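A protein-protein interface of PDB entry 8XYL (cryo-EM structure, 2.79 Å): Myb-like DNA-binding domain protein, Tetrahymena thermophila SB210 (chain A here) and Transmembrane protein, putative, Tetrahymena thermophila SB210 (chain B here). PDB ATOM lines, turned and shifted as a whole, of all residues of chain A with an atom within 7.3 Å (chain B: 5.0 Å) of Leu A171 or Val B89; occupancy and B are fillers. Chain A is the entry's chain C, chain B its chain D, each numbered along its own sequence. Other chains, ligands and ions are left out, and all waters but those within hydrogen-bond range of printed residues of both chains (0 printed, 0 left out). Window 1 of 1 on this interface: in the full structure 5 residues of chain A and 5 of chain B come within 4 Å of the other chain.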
ATOM      1  N   PHE A 165       4.219   0.547  11.787  1.00  0.00           N
ATOM      2  CA  PHE A 165       4.751   1.421  12.820  1.00  0.00           C
ATOM      3  C   PHE A 165       3.898   2.676  12.952  1.00  0.00           C
ATOM      4  O   PHE A 165       3.272   3.133  11.991  1.00  0.00           O
ATOM      5  CB  PHE A 165       6.193   1.812  12.492  1.00  0.00           C
ATOM      6  CG  PHE A 165       7.179   0.692  12.634  1.00  0.00           C
ATOM      7  CD1 PHE A 165       7.188  -0.105  13.766  1.00  0.00           C
ATOM      8  CD2 PHE A 165       8.115   0.449  11.642  1.00  0.00           C
ATOM      9  CE1 PHE A 165       8.103  -1.133  13.899  1.00  0.00           C
ATOM     10  CE2 PHE A 165       9.031  -0.575  11.767  1.00  0.00           C
ATOM     11  CZ  PHE A 165       9.025  -1.368  12.897  1.00  0.00           C
ATOM     12  N   THR A 166       3.879   3.241  14.157  1.00  0.00           N
ATOM     13  CA  THR A 166       3.188   4.500  14.383  1.00  0.00           C
ATOM     14  C   THR A 166       4.000   5.656  13.798  1.00  0.00           C
ATOM     15  O   THR A 166       5.139   5.495  13.352  1.00  0.00           O
ATOM     16  CB  THR A 166       2.929   4.717  15.872  1.00  0.00           C
ATOM     17  OG1 THR A 166       4.146   5.098  16.524  1.00  0.00           O
ATOM     18  CG2 THR A 166       2.380   3.450  16.510  1.00  0.00           C
ATOM     19  N   ASN A 167       3.400   6.844  13.814  1.00  0.00           N
ATOM     20  CA  ASN A 167       3.965   8.002  13.136  1.00  0.00           C
ATOM     21  C   ASN A 167       5.169   8.596  13.854  1.00  0.00           C
ATOM     22  O   ASN A 167       5.852   9.445  13.273  1.00  0.00           O
ATOM     23  CB  ASN A 167       2.887   9.069  12.968  1.00  0.00           C
ATOM     24  CG  ASN A 167       1.922   8.741  11.854  1.00  0.00           C
ATOM     25  OD1 ASN A 167       1.510   7.592  11.695  1.00  0.00           O
ATOM     26  ND2 ASN A 167       1.548   9.745  11.080  1.00  0.00           N
ATOM     27  N   LEU A 168       5.443   8.181  15.091  1.00  0.00           N
ATOM     28  CA  LEU A 168       6.602   8.657  15.837  1.00  0.00           C
ATOM     29  C   LEU A 168       7.805   7.735  15.717  1.00  0.00           C
ATOM     30  O   LEU A 168       8.937   8.216  15.595  1.00  0.00           O
ATOM     31  CB  LEU A 168       6.245   8.832  17.315  1.00  0.00           C
ATOM     32  CG  LEU A 168       7.310   9.507  18.179  1.00  0.00           C
ATOM     33  CD1 LEU A 168       7.803  10.796  17.538  1.00  0.00           C
ATOM     34  CD2 LEU A 168       6.772   9.762  19.570  1.00  0.00           C
ATOM     35  N   GLU A 169       7.595   6.416  15.754  1.00  0.00           N
ATOM     36  CA  GLU A 169       8.709   5.499  15.536  1.00  0.00           C
ATOM     37  C   GLU A 169       9.195   5.559  14.092  1.00  0.00           C
ATOM     38  O   GLU A 169      10.402   5.465  13.835  1.00  0.00           O
ATOM     39  CB  GLU A 169       8.316   4.075  15.925  1.00  0.00           C
ATOM     40  CG  GLU A 169       6.924   3.661  15.516  1.00  0.00           C
ATOM     41  CD  GLU A 169       6.362   2.572  16.410  1.00  0.00           C
ATOM     42  OE1 GLU A 169       6.994   2.266  17.443  1.00  0.00           O
ATOM     43  OE2 GLU A 169       5.298   2.014  16.077  1.00  0.00           O
ATOM     44  N   ILE A 170       8.271   5.739  13.143  1.00  0.00           N
ATOM     45  CA  ILE A 170       8.653   6.009  11.759  1.00  0.00           C
ATOM     46  C   ILE A 170       9.501   7.271  11.685  1.00  0.00           C
ATOM     47  O   ILE A 170      10.529   7.312  10.996  1.00  0.00           O
ATOM     48  CB  ILE A 170       7.395   6.117  10.874  1.00  0.00           C
ATOM     49  CG1 ILE A 170       6.913   4.733  10.447  1.00  0.00           C
ATOM     50  CG2 ILE A 170       7.654   6.972   9.643  1.00  0.00           C
ATOM     51  CD1 ILE A 170       5.492   4.717   9.925  1.00  0.00           C
ATOM     52  N   LEU A 171       9.102   8.308  12.426  1.00  0.00           N
ATOM     53  CA  LEU A 171       9.794   9.590  12.377  1.00  0.00           C
ATOM     54  C   LEU A 171      11.202   9.484  12.957  1.00  0.00           C
ATOM     55  O   LEU A 171      12.155  10.032  12.390  1.00  0.00           O
ATOM     56  CB  LEU A 171       8.959  10.635  13.122  1.00  0.00           C
ATOM     57  CG  LEU A 171       8.960  12.116  12.731  1.00  0.00           C
ATOM     58  CD1 LEU A 171      10.297  12.788  12.924  1.00  0.00           C
ATOM     59  CD2 LEU A 171       8.492  12.275  11.294  1.00  0.00           C
ATOM     60  N   THR A 172      11.362   8.762  14.070  1.00  0.00           N
ATOM     61  CA  THR A 172      12.697   8.647  14.652  1.00  0.00           C
ATOM     62  C   THR A 172      13.582   7.689  13.858  1.00  0.00           C
ATOM     63  O   THR A 172      14.798   7.901  13.785  1.00  0.00           O
ATOM     64  CB  THR A 172      12.635   8.232  16.127  1.00  0.00           C
ATOM     65  OG1 THR A 172      13.967   8.100  16.637  1.00  0.00           O
ATOM     66  CG2 THR A 172      11.926   6.919  16.310  1.00  0.00           C
ATOM     67  N   HIS A 173      13.004   6.655  13.233  1.00  0.00           N
ATOM     68  CA  HIS A 173      13.782   5.822  12.320  1.00  0.00           C
ATOM     69  C   HIS A 173      14.260   6.631  11.124  1.00  0.00           C
ATOM     70  O   HIS A 173      15.409   6.488  10.685  1.00  0.00           O
ATOM     71  CB  HIS A 173      12.950   4.628  11.853  1.00  0.00           C
ATOM     72  CG  HIS A 173      12.822   3.540  12.873  1.00  0.00           C
ATOM     73  ND1 HIS A 173      11.774   2.646  12.878  1.00  0.00           N
ATOM     74  CD2 HIS A 173      13.610   3.202  13.921  1.00  0.00           C
ATOM     75  CE1 HIS A 173      11.920   1.805  13.886  1.00  0.00           C
ATOM     76  NE2 HIS A 173      13.026   2.120  14.535  1.00  0.00           N
ATOM     77  N   LEU A 174      13.390   7.492  10.590  1.00  0.00           N
ATOM     78  CA  LEU A 174      13.761   8.352   9.473  1.00  0.00           C
ATOM     79  C   LEU A 174      14.866   9.323   9.871  1.00  0.00           C
ATOM     80  O   LEU A 174      15.805   9.561   9.103  1.00  0.00           O
ATOM     81  CB  LEU A 174      12.526   9.104   8.980  1.00  0.00           C
ATOM     82  CG  LEU A 174      11.781   8.594   7.743  1.00  0.00           C
ATOM     83  CD1 LEU A 174      11.540   7.096   7.813  1.00  0.00           C
ATOM     84  CD2 LEU A 174      10.462   9.334   7.582  1.00  0.00           C
ATOM     85  N   TYR A 175      14.770   9.890  11.078  1.00  0.00           N
ATOM     86  CA  TYR A 175      15.808  10.801  11.555  1.00  0.00           C
ATOM     87  C   TYR A 175      17.138  10.085  11.759  1.00  0.00           C
ATOM     88  O   TYR A 175      18.198  10.626  11.423  1.00  0.00           O
ATOM     89  CB  TYR A 175      15.364  11.484  12.848  1.00  0.00           C
ATOM     90  CG  TYR A 175      14.985  12.934  12.663  1.00  0.00           C
ATOM     91  CD1 TYR A 175      15.929  13.943  12.803  1.00  0.00           C
ATOM     92  CD2 TYR A 175      13.689  13.294  12.336  1.00  0.00           C
ATOM     93  CE1 TYR A 175      15.585  15.273  12.629  1.00  0.00           C
ATOM     94  CE2 TYR A 175      13.333  14.617  12.161  1.00  0.00           C
ATOM     95  CZ  TYR A 175      14.284  15.602  12.307  1.00  0.00           C
ATOM     96  OH  TYR A 175      13.931  16.920  12.131  1.00  0.00           O
ATOM     97  N   ASN A 176      17.105   8.869  12.314  1.00  0.00           N
ATOM     98  CA  ASN A 176      18.335   8.105  12.504  1.00  0.00           C
ATOM     99  C   ASN A 176      18.974   7.753  11.167  1.00  0.00           C
ATOM    100  O   ASN A 176      20.198   7.855  11.004  1.00  0.00           O
ATOM    101  CB  ASN A 176      18.045   6.841  13.314  1.00  0.00           C
ATOM    102  CG  ASN A 176      17.995   7.104  14.805  1.00  0.00           C
ATOM    103  OD1 ASN A 176      17.073   6.665  15.493  1.00  0.00           O
ATOM    104  ND2 ASN A 176      18.990   7.822  15.313  1.00  0.00           N
ATOM    105  N   LEU A 177      18.154   7.344  10.193  1.00  0.00           N
ATOM    106  CA  LEU A 177      18.665   7.031   8.863  1.00  0.00           C
ATOM    107  C   LEU A 177      19.275   8.264   8.207  1.00  0.00           C
ATOM    108  O   LEU A 177      20.357   8.181   7.613  1.00  0.00           O
ATOM    109  CB  LEU A 177      17.540   6.448   8.003  1.00  0.00           C
ATOM    110  CG  LEU A 177      17.812   5.697   6.689  1.00  0.00           C
ATOM    111  CD1 LEU A 177      16.628   4.798   6.378  1.00  0.00           C
ATOM    112  CD2 LEU A 177      18.074   6.619   5.503  1.00  0.00           C
ATOM    113  N   ASN B  87      12.734  10.851  24.391  1.00  0.00           N
ATOM    114  CA  ASN B  87      12.877  10.758  22.941  1.00  0.00           C
ATOM    115  C   ASN B  87      13.311  12.116  22.402  1.00  0.00           C
ATOM    116  O   ASN B  87      12.550  13.089  22.469  1.00  0.00           O
ATOM    117  CB  ASN B  87      11.571  10.298  22.297  1.00  0.00           C
ATOM    118  CG  ASN B  87      11.790   9.593  20.975  1.00  0.00           C
ATOM    119  OD1 ASN B  87      12.876   9.649  20.401  1.00  0.00           O
ATOM    120  ND2 ASN B  87      10.756   8.918  20.486  1.00  0.00           N
ATOM    121  N   ILE B  88      14.531  12.168  21.861  1.00  0.00           N
ATOM    122  CA  ILE B  88      15.079  13.413  21.328  1.00  0.00           C
ATOM    123  C   ILE B  88      14.231  13.904  20.161  1.00  0.00           C
ATOM    124  O   ILE B  88      14.019  15.110  19.983  1.00  0.00           O
ATOM    125  CB  ILE B  88      16.546  13.210  20.904  1.00  0.00           C
ATOM    126  CG1 ILE B  88      17.361  12.614  22.051  1.00  0.00           C
ATOM    127  CG2 ILE B  88      17.165  14.523  20.448  1.00  0.00           C
ATOM    128  CD1 ILE B  88      17.547  13.547  23.211  1.00  0.00           C
ATOM    129  N   VAL B  89      13.739  12.969  19.347  1.00  0.00           N
ATOM    130  CA  VAL B  89      12.889  13.318  18.215  1.00  0.00           C
ATOM    131  C   VAL B  89      11.570  13.911  18.697  1.00  0.00           C
ATOM    132  O   VAL B  89      11.096  14.923  18.163  1.00  0.00           O
ATOM    133  CB  VAL B  89      12.674  12.079  17.325  1.00  0.00           C
ATOM    134  CG1 VAL B  89      11.511  12.284  16.376  1.00  0.00           C
ATOM    135  CG2 VAL B  89      13.945  11.765  16.557  1.00  0.00           C
ATOM    136  N   GLU B  90      10.962  13.303  19.721  1.00  0.00           N
ATOM    137  CA  GLU B  90       9.687  13.806  20.220  1.00  0.00           C
ATOM    138  C   GLU B  90       9.849  15.168  20.882  1.00  0.00           C
ATOM    139  O   GLU B  90       8.952  16.012  20.793  1.00  0.00           O
ATOM    140  CB  GLU B  90       9.051  12.805  21.188  1.00  0.00           C
ATOM    141  CG  GLU B  90       7.712  13.273  21.758  1.00  0.00           C
ATOM    142  CD  GLU B  90       6.788  12.136  22.145  1.00  0.00           C
ATOM    143  OE1 GLU B  90       7.201  11.272  22.945  1.00  0.00           O
ATOM    144  OE2 GLU B  90       5.638  12.118  21.658  1.00  0.00           O
ATOM    145  N   LEU B  91      10.990  15.413  21.535  1.00  0.00           N
ATOM    146  CA  LEU B  91      11.232  16.739  22.102  1.00  0.00           C
ATOM    147  C   LEU B  91      11.255  17.808  21.014  1.00  0.00           C
ATOM    148  O   LEU B  91      10.647  18.874  21.163  1.00  0.00           O
ATOM    149  CB  LEU B  91      12.540  16.754  22.891  1.00  0.00           C
ATOM    150  CG  LEU B  91      12.588  15.896  24.153  1.00  0.00           C
ATOM    151  CD1 LEU B  91      13.817  16.231  24.980  1.00  0.00           C
ATOM    152  CD2 LEU B  91      11.324  16.068  24.960  1.00  0.00           C
ATOM    153  N   GLU B  92      11.924  17.518  19.897  1.00  0.00           N
ATOM    154  CA  GLU B  92      11.962  18.458  18.780  1.00  0.00           C
ATOM    155  C   GLU B  92      10.580  18.646  18.165  1.00  0.00           C
ATOM    156  O   GLU B  92      10.181  19.772  17.843  1.00  0.00           O
ATOM    157  CB  GLU B  92      12.956  17.971  17.726  1.00  0.00           C
ATOM    158  CG  GLU B  92      13.027  18.848  16.490  1.00  0.00           C
ATOM    159  CD  GLU B  92      13.861  18.230  15.390  1.00  0.00           C
ATOM    160  OE1 GLU B  92      13.525  17.113  14.948  1.00  0.00           O
ATOM    161  OE2 GLU B  92      14.851  18.862  14.968  1.00  0.00           O
ATOM    162  N   LEU B  93       9.833  17.551  17.997  1.00  0.00           N
ATOM    163  CA  LEU B  93       8.507  17.636  17.387  1.00  0.00           C
ATOM    164  C   LEU B  93       7.549  18.452  18.247  1.00  0.00           C
ATOM    165  O   LEU B  93       6.805  19.299  17.740  1.00  0.00           O
ATOM    166  CB  LEU B  93       7.948  16.235  17.146  1.00  0.00           C
ATOM    167  CG  LEU B  93       8.638  15.384  16.079  1.00  0.00           C
ATOM    168  CD1 LEU B  93       7.810  14.154  15.759  1.00  0.00           C
ATOM    169  CD2 LEU B  93       8.887  16.199  14.824  1.00  0.00           C
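Among the printed residues, merely in contact across the chains: Leu A168 with Glu B90 (3.3 Å), Leu A168 with Leu B93 (3.8 Å), Leu A171 with Val B89 (3.7 Å), Leu A171 with Leu B93 (3.8 Å), Thr A172 with Val B89 (3.7 Å) and Tyr A175 with Val B89 (3.98 Å).
OH of Tyr A175 sits at hydrogen-bond distance from OE1 of Glu B92 (2.9 Å).
Hydrophobic or aromatic side chains of chain B that line the printed part of chain A: Val B89 and Leu B93. Hydrophobic or aromatic side chains of chain A within 4 Å of the printed part of chain B: Leu A168, Leu A171 and Tyr A175. Among the printed residues, no Asp or Glu carboxylate lies within 4 Å of a Lys or Arg side-chain nitrogen of the other chain.
The backbone carbonyl oxygen of Thr A172 lies close to the side-chain amide oxygen of Asn A176 (3.1 Å).
Leu A171 touches two residues of chain B. Of the printed residues of chain A, Val B89 touches Leu A171 (3.7 Å), Thr A172 (3.7 Å) and Tyr A175 (3.98 Å). Of the printed residues of chain A, Glu B90 touches Leu A168 (3.3 Å). Of the printed residues of chain A, Glu B92 touches Tyr A175. Of the printed residues of chain A, Leu B93 touches Leu A168 (3.8 Å) and Leu A171 (3.8 Å). The nearest printed residue of chain A that does not touch Val B89 is Leu A168 (4.2 Å). The nearest printed residue of chain A that does not touch Glu B92 is Leu A171 (5.8 Å).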
